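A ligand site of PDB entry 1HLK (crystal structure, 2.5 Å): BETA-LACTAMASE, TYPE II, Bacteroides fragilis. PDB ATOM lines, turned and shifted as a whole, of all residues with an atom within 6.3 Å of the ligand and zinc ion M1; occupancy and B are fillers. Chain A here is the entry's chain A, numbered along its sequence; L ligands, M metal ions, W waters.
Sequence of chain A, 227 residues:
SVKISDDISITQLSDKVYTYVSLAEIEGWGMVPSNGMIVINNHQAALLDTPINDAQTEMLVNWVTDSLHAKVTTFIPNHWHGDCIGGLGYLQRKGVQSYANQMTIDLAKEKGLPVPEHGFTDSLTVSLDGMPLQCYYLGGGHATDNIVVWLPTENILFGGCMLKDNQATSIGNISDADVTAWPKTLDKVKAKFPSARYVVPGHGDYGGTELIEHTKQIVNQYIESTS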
ATOM      1  N   ILE A  26      13.392 -18.475  29.160  1.00  0.00           N
ATOM      2  CA  ILE A  26      14.294 -18.198  30.261  1.00  0.00           C
ATOM      3  C   ILE A  26      13.529 -17.440  31.341  1.00  0.00           C
ATOM      4  O   ILE A  26      12.986 -16.369  31.075  1.00  0.00           O
ATOM      5  CB  ILE A  26      15.504 -17.348  29.826  1.00  0.00           C
ATOM      6  CG1 ILE A  26      16.348 -18.117  28.807  1.00  0.00           C
ATOM      7  CG2 ILE A  26      16.357 -16.982  31.034  1.00  0.00           C
ATOM      8  CD1 ILE A  26      17.576 -17.366  28.354  1.00  0.00           C
ATOM      9  N   TRP A  29      12.967 -13.589  31.395  1.00  0.00           N
ATOM     10  CA  TRP A  29      13.092 -12.954  30.093  1.00  0.00           C
ATOM     11  C   TRP A  29      12.148 -13.520  29.034  1.00  0.00           C
ATOM     12  O   TRP A  29      12.046 -12.972  27.936  1.00  0.00           O
ATOM     13  CB  TRP A  29      14.541 -13.046  29.586  1.00  0.00           C
ATOM     14  CG  TRP A  29      15.542 -12.594  30.593  1.00  0.00           C
ATOM     15  CD1 TRP A  29      16.032 -13.312  31.656  1.00  0.00           C
ATOM     16  CD2 TRP A  29      16.114 -11.278  30.705  1.00  0.00           C
ATOM     17  NE1 TRP A  29      16.861 -12.529  32.419  1.00  0.00           N
ATOM     18  CE2 TRP A  29      16.933 -11.275  31.857  1.00  0.00           C
ATOM     19  CE3 TRP A  29      16.014 -10.107  29.944  1.00  0.00           C
ATOM     20  CZ2 TRP A  29      17.646 -10.149  32.273  1.00  0.00           C
ATOM     21  CZ3 TRP A  29      16.727  -8.982  30.360  1.00  0.00           C
ATOM     22  CH2 TRP A  29      17.530  -9.015  31.521  1.00  0.00           C
ATOM     23  N   MET A  31      10.416 -15.913  26.092  1.00  0.00           N
ATOM     24  CA  MET A  31      10.906 -16.414  24.806  1.00  0.00           C
ATOM     25  C   MET A  31      12.132 -15.628  24.330  1.00  0.00           C
ATOM     26  O   MET A  31      12.038 -14.437  24.043  1.00  0.00           O
ATOM     27  CB  MET A  31       9.804 -16.307  23.731  1.00  0.00           C
ATOM     28  CG  MET A  31       8.765 -17.420  23.723  1.00  0.00           C
ATOM     29  SD  MET A  31       9.451 -19.001  23.152  1.00  0.00           S
ATOM     30  CE  MET A  31      10.081 -18.531  21.527  1.00  0.00           C
ATOM     31  N   VAL A  32      13.277 -16.294  24.255  1.00  0.00           N
ATOM     32  CA  VAL A  32      14.472 -15.605  23.796  1.00  0.00           C
ATOM     33  C   VAL A  32      15.346 -16.457  22.888  1.00  0.00           C
ATOM     34  O   VAL A  32      15.778 -17.544  23.262  1.00  0.00           O
ATOM     35  CB  VAL A  32      15.310 -15.097  24.990  1.00  0.00           C
ATOM     36  CG1 VAL A  32      14.485 -14.145  25.829  1.00  0.00           C
ATOM     37  CG2 VAL A  32      15.772 -16.264  25.831  1.00  0.00           C
ATOM     38  N   SER A  34      18.593 -17.742  20.958  1.00  0.00           N
ATOM     39  CA  SER A  34      20.024 -17.820  21.236  1.00  0.00           C
ATOM     40  C   SER A  34      20.779 -18.298  20.000  1.00  0.00           C
ATOM     41  O   SER A  34      20.383 -19.292  19.382  1.00  0.00           O
ATOM     42  CB  SER A  34      20.318 -18.778  22.397  1.00  0.00           C
ATOM     43  OG  SER A  34      19.802 -18.276  23.614  1.00  0.00           O
ATOM     44  N   HIS A  79      30.946 -18.889  26.853  1.00  0.00           N
ATOM     45  CA  HIS A  79      31.136 -18.711  28.292  1.00  0.00           C
ATOM     46  C   HIS A  79      30.226 -19.695  29.056  1.00  0.00           C
ATOM     47  O   HIS A  79      29.486 -20.464  28.438  1.00  0.00           O
ATOM     48  CB  HIS A  79      30.915 -17.250  28.740  1.00  0.00           C
ATOM     49  CG  HIS A  79      29.588 -16.676  28.388  1.00  0.00           C
ATOM     50  ND1 HIS A  79      29.187 -16.463  27.083  1.00  0.00           N
ATOM     51  CD2 HIS A  79      28.539 -16.304  29.157  1.00  0.00           C
ATOM     52  CE1 HIS A  79      27.948 -15.983  27.072  1.00  0.00           C
ATOM     53  NE2 HIS A  79      27.538 -15.878  28.321  1.00  0.00           N
ATOM     54  N   HIS A  81      27.345 -19.649  30.637  1.00  0.00           N
ATOM     55  CA  HIS A  81      25.885 -19.598  30.701  1.00  0.00           C
ATOM     56  C   HIS A  81      25.148 -20.687  29.951  1.00  0.00           C
ATOM     57  O   HIS A  81      25.710 -21.371  29.093  1.00  0.00           O
ATOM     58  CB  HIS A  81      25.355 -18.227  30.279  1.00  0.00           C
ATOM     59  CG  HIS A  81      25.535 -17.173  31.322  1.00  0.00           C
ATOM     60  ND1 HIS A  81      25.413 -15.822  31.042  1.00  0.00           N
ATOM     61  CD2 HIS A  81      25.810 -17.257  32.639  1.00  0.00           C
ATOM     62  CE1 HIS A  81      25.604 -15.132  32.153  1.00  0.00           C
ATOM     63  NE2 HIS A  81      25.852 -15.976  33.136  1.00  0.00           N
ATOM     64  N   ASP A  83      22.943 -20.658  27.614  1.00  0.00           N
ATOM     65  CA  ASP A  83      22.894 -20.540  26.171  1.00  0.00           C
ATOM     66  C   ASP A  83      24.244 -20.735  25.470  1.00  0.00           C
ATOM     67  O   ASP A  83      24.447 -20.293  24.334  1.00  0.00           O
ATOM     68  CB  ASP A  83      22.251 -19.198  25.789  1.00  0.00           C
ATOM     69  CG  ASP A  83      22.832 -18.012  26.535  1.00  0.00           C
ATOM     70  OD1 ASP A  83      22.854 -18.052  27.788  1.00  0.00           O
ATOM     71  OD2 ASP A  83      23.253 -17.034  25.875  1.00  0.00           O
ATOM     72  N   CYS A  84      25.161 -21.418  26.148  1.00  0.00           N
ATOM     73  CA  CYS A  84      26.476 -21.707  25.584  1.00  0.00           C
ATOM     74  C   CYS A  84      26.830 -23.192  25.776  1.00  0.00           C
ATOM     75  O   CYS A  84      27.214 -23.872  24.820  1.00  0.00           O
ATOM     76  CB  CYS A  84      27.534 -20.809  26.215  1.00  0.00           C
ATOM     77  SG  CYS A  84      27.209 -19.044  26.060  1.00  0.00           S
ATOM     78  N   HIS A 142      30.421  -9.170  28.791  1.00  0.00           N
ATOM     79  CA  HIS A 142      29.106  -9.669  29.174  1.00  0.00           C
ATOM     80  C   HIS A 142      29.290 -10.589  30.365  1.00  0.00           C
ATOM     81  O   HIS A 142      28.478 -10.626  31.280  1.00  0.00           O
ATOM     82  CB  HIS A 142      28.476 -10.464  28.041  1.00  0.00           C
ATOM     83  CG  HIS A 142      27.368 -11.353  28.492  1.00  0.00           C
ATOM     84  ND1 HIS A 142      26.170 -10.876  28.955  1.00  0.00           N
ATOM     85  CD2 HIS A 142      27.317 -12.702  28.645  1.00  0.00           C
ATOM     86  CE1 HIS A 142      25.429 -11.877  29.381  1.00  0.00           C
ATOM     87  NE2 HIS A 142      26.096 -13.004  29.199  1.00  0.00           N
ATOM     88  N   GLY A 160      29.620 -13.738  20.302  1.00  0.00           N
ATOM     89  CA  GLY A 160      28.889 -14.130  21.497  1.00  0.00           C
ATOM     90  C   GLY A 160      28.066 -12.979  22.045  1.00  0.00           C
ATOM     91  O   GLY A 160      27.707 -12.040  21.329  1.00  0.00           O
ATOM     92  N   CYS A 161      27.775 -13.027  23.330  1.00  0.00           N
ATOM     93  CA  CYS A 161      26.960 -12.017  23.963  1.00  0.00           C
ATOM     94  C   CYS A 161      27.686 -10.745  24.334  1.00  0.00           C
ATOM     95  O   CYS A 161      27.085  -9.807  24.871  1.00  0.00           O
ATOM     96  CB  CYS A 161      26.259 -12.629  25.193  1.00  0.00           C
ATOM     97  SG  CYS A 161      25.226 -14.061  24.745  1.00  0.00           S
ATOM     98  N   LYS A 164      26.086  -6.967  21.003  1.00  0.00           N
ATOM     99  CA  LYS A 164      24.633  -6.824  20.837  1.00  0.00           C
ATOM    100  C   LYS A 164      24.286  -6.564  19.364  1.00  0.00           C
ATOM    101  O   LYS A 164      25.154  -6.134  18.592  1.00  0.00           O
ATOM    102  CB  LYS A 164      24.109  -5.643  21.666  1.00  0.00           C
ATOM    103  CG  LYS A 164      23.543  -5.972  23.025  1.00  0.00           C
ATOM    104  CD  LYS A 164      24.570  -6.375  24.017  1.00  0.00           C
ATOM    105  CE  LYS A 164      23.913  -6.486  25.399  1.00  0.00           C
ATOM    106  NZ  LYS A 164      22.771  -7.438  25.447  1.00  0.00           N
ATOM    107  N   ASP A 165      23.032  -6.814  18.980  1.00  0.00           N
ATOM    108  CA  ASP A 165      22.611  -6.576  17.600  1.00  0.00           C
ATOM    109  C   ASP A 165      22.092  -5.159  17.433  1.00  0.00           C
ATOM    110  O   ASP A 165      21.612  -4.545  18.393  1.00  0.00           O
ATOM    111  CB  ASP A 165      21.560  -7.619  17.136  1.00  0.00           C
ATOM    112  CG  ASP A 165      20.203  -7.458  17.799  1.00  0.00           C
ATOM    113  OD1 ASP A 165      20.110  -7.554  19.045  1.00  0.00           O
ATOM    114  OD2 ASP A 165      19.209  -7.254  17.078  1.00  0.00           O
ATOM    115  N   ALA A 168      19.087  -3.465  19.241  1.00  0.00           N
ATOM    116  CA  ALA A 168      19.055  -3.514  20.688  1.00  0.00           C
ATOM    117  C   ALA A 168      19.291  -2.128  21.278  1.00  0.00           C
ATOM    118  O   ALA A 168      20.160  -1.377  20.834  1.00  0.00           O
ATOM    119  CB  ALA A 168      20.095  -4.490  21.206  1.00  0.00           C
ATOM    120  N   THR A 169      18.508  -1.798  22.302  1.00  0.00           N
ATOM    121  CA  THR A 169      18.607  -0.513  22.967  1.00  0.00           C
ATOM    122  C   THR A 169      18.896  -0.720  24.444  1.00  0.00           C
ATOM    123  O   THR A 169      19.201   0.225  25.183  1.00  0.00           O
ATOM    124  CB  THR A 169      17.290   0.259  22.800  1.00  0.00           C
ATOM    125  OG1 THR A 169      16.217  -0.481  23.394  1.00  0.00           O
ATOM    126  CG2 THR A 169      16.989   0.460  21.320  1.00  0.00           C
ATOM    127  N   SER A 170      18.797  -1.973  24.873  1.00  0.00           N
ATOM    128  CA  SER A 170      19.049  -2.369  26.264  1.00  0.00           C
ATOM    129  C   SER A 170      20.424  -3.030  26.402  1.00  0.00           C
ATOM    130  O   SER A 170      20.953  -3.584  25.455  1.00  0.00           O
ATOM    131  CB  SER A 170      17.962  -3.341  26.725  1.00  0.00           C
ATOM    132  OG  SER A 170      18.311  -3.955  27.959  1.00  0.00           O
ATOM    133  N   ILE A 171      20.990  -2.947  27.599  1.00  0.00           N
ATOM    134  CA  ILE A 171      22.298  -3.545  27.831  1.00  0.00           C
ATOM    135  C   ILE A 171      22.129  -5.023  28.151  1.00  0.00           C
ATOM    136  O   ILE A 171      23.078  -5.801  28.082  1.00  0.00           O
ATOM    137  CB  ILE A 171      23.040  -2.824  28.975  1.00  0.00           C
ATOM    138  CG1 ILE A 171      24.379  -3.516  29.233  1.00  0.00           C
ATOM    139  CG2 ILE A 171      22.177  -2.770  30.223  1.00  0.00           C
ATOM    140  CD1 ILE A 171      25.234  -2.841  30.285  1.00  0.00           C
ATOM    141  N   GLY A 172      20.887  -5.401  28.490  1.00  0.00           N
ATOM    142  CA  GLY A 172      20.573  -6.790  28.805  1.00  0.00           C
ATOM    143  C   GLY A 172      20.927  -7.326  30.180  1.00  0.00           C
ATOM    144  O   GLY A 172      21.003  -6.588  31.168  1.00  0.00           O
ATOM    145  N   ASN A 173      21.150  -8.635  30.232  1.00  0.00           N
ATOM    146  CA  ASN A 173      21.495  -9.344  31.469  1.00  0.00           C
ATOM    147  C   ASN A 173      22.936  -9.099  31.922  1.00  0.00           C
ATOM    148  O   ASN A 173      23.854  -9.800  31.509  1.00  0.00           O
ATOM    149  CB  ASN A 173      21.275 -10.846  31.272  1.00  0.00           C
ATOM    150  CG  ASN A 173      21.653 -11.656  32.498  1.00  0.00           C
ATOM    151  OD1 ASN A 173      21.117 -11.444  33.588  1.00  0.00           O
ATOM    152  ND2 ASN A 173      22.579 -12.592  32.328  1.00  0.00           N
ATOM    153  N   ILE A 174      23.126  -8.114  32.809  1.00  0.00           N
ATOM    154  CA  ILE A 174      24.451  -7.813  33.307  1.00  0.00           C
ATOM    155  C   ILE A 174      24.738  -8.386  34.702  1.00  0.00           C
ATOM    156  O   ILE A 174      25.441  -7.775  35.492  1.00  0.00           O
ATOM    157  CB  ILE A 174      24.678  -6.286  33.350  1.00  0.00           C
ATOM    158  CG1 ILE A 174      23.708  -5.639  34.334  1.00  0.00           C
ATOM    159  CG2 ILE A 174      24.484  -5.702  31.980  1.00  0.00           C
ATOM    160  CD1 ILE A 174      23.940  -4.143  34.489  1.00  0.00           C
ATOM    161  N   GLY A 202      25.499 -12.905  20.178  1.00  0.00           N
ATOM    162  CA  GLY A 202      24.918 -13.994  20.932  1.00  0.00           C
ATOM    163  C   GLY A 202      23.392 -14.011  20.890  1.00  0.00           C
ATOM    164  O   GLY A 202      22.783 -15.019  21.241  1.00  0.00           O
ATOM    165  N   HIS A 203      22.799 -12.897  20.473  1.00  0.00           N
ATOM    166  CA  HIS A 203      21.350 -12.762  20.377  1.00  0.00           C
ATOM    167  C   HIS A 203      21.048 -11.693  19.339  1.00  0.00           C
ATOM    168  O   HIS A 203      21.600 -10.606  19.412  1.00  0.00           O
ATOM    169  CB  HIS A 203      20.733 -12.323  21.717  1.00  0.00           C
ATOM    170  CG  HIS A 203      20.905 -13.333  22.817  1.00  0.00           C
ATOM    171  ND1 HIS A 203      20.197 -14.515  22.865  1.00  0.00           N
ATOM    172  CD2 HIS A 203      21.727 -13.348  23.889  1.00  0.00           C
ATOM    173  CE1 HIS A 203      20.587 -15.216  23.913  1.00  0.00           C
ATOM    174  NE2 HIS A 203      21.511 -14.528  24.549  1.00  0.00           N
HETATM  175  C1  LIG L   1      19.598 -13.712  28.826  1.00  0.00           C
HETATM  176  C2  LIG L   1      18.403 -13.131  28.402  1.00  0.00           C
HETATM  177  C3  LIG L   1      18.433 -12.153  27.422  1.00  0.00           C
HETATM  178  C4  LIG L   1      19.664 -11.699  26.901  1.00  0.00           C
HETATM  179  C5  LIG L   1      20.856 -12.040  27.593  1.00  0.00           C
HETATM  180  C6  LIG L   1      20.824 -13.118  28.500  1.00  0.00           C
HETATM  181  O1  LIG L   1      17.242 -11.629  26.957  1.00  0.00           O
HETATM  182  C7  LIG L   1      17.201 -10.643  25.993  1.00  0.00           C
HETATM  183  C8  LIG L   1      18.299 -10.253  25.306  1.00  0.00           C
HETATM  184  C9  LIG L   1      19.616 -10.905  25.652  1.00  0.00           C
HETATM  185  C10 LIG L   1      15.846 -10.039  25.780  1.00  0.00           C
HETATM  186  C11 LIG L   1      15.949  -8.637  25.164  1.00  0.00           C
HETATM  187  O2  LIG L   1      16.887  -8.623  24.082  1.00  0.00           O
HETATM  188  C12 LIG L   1      18.200  -9.187  24.221  1.00  0.00           C
HETATM  189  O3  LIG L   1      21.945 -13.651  29.126  1.00  0.00           O
HETATM  190  O4  LIG L   1      19.647 -14.880  29.557  1.00  0.00           O
HETATM  191  C13 LIG L   1      22.125 -11.312  27.401  1.00  0.00           C
HETATM  192  O5  LIG L   1      23.008 -11.915  26.576  1.00  0.00           O
HETATM  193  O6  LIG L   1      19.209  -8.183  24.309  1.00  0.00           O
HETATM  194  C14 LIG L   1      19.106  -7.114  25.231  1.00  0.00           C
HETATM  195  C15 LIG L   1      14.612  -8.099  24.643  1.00  0.00           C
HETATM  196  O7  LIG L   1      22.343 -10.251  27.928  1.00  0.00           O
HETATM  197  O8  LIG L   1      20.552 -10.765  24.893  1.00  0.00           O
HETATM  198 ZN    ZN M   1      23.706 -14.338  26.176  1.00  0.00          ZN
HETATM  199 ZN    ZN M   2      25.525 -15.120  28.861  1.00  0.00          ZN
HETATM  200  O   HOH W   1      17.841  -5.058  23.229  1.00  0.00           O
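O7 of the ligand lies within hydrogen-bond range of N of Asn 173, 3.1 Å away.
O3 of the ligand is in hydrogen-bond range of ND2 of Asn 173, at 3.4 Å.
The side-chain amino group of Lys 164 is in salt-bridge range of an oxygen (O7) of the ligand (3.8 Å).
CD1 of Ile 26 touches O4 of the ligand (3.5 Å).
Trp 29 touches the ligand.
CG1 of Val 32 touches O1 of the ligand, at 3.9 Å.
His 142 touches the ligand (CE1 to O5, 3.7 Å).
O of Ser 170 touches C14 of the ligand, 3.99 Å away.
CA of Gly 172 touches C14 of the ligand (3.9 Å).
Hydrophobic or aromatic side chains that line the ligand: Ile 26, Trp 29, Val 32, His 142 and His 203.
Of the 23 residues printed, 10 come within 4 Å of the ligand.
The nearest printed residue that does not touch the ligand is Ile 171 (4.5 Å).
Three residues have an atom within 4 Å of zinc ion M1: Asp 83, Cys 161 and His 203.
The nearest printed residue that does not touch zinc ion M1 is His 142 (4.1 Å).
NE2 of His 203 lies close to SG of Cys 161 (3.7 Å).
SG of Cys 161 lies close to OD2 of Asp 83.
NE2 of His 203 sits at hydrogen-bond distance from OD2 of Asp 83.
The side-chain amino group (NZ) of Lys 164 lies close to the backbone carbonyl oxygen (O) of Ile 171 (3.1 Å).
The backbone NH (N) of Gly 172 is in hydrogen-bond range of the side-chain hydroxyl (OG) of Ser 170 (3.0 Å).
Zinc ion M1 is bound by SG of Cys 161 (2.1 Å) and O5 of the ligand (2.6 Å).
Slightly farther from zinc ion M1 lies NE2 of His 203 (2.7 Å).
Slightly farther from zinc ion M1 lies OD2 of Asp 83 (2.8 Å).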
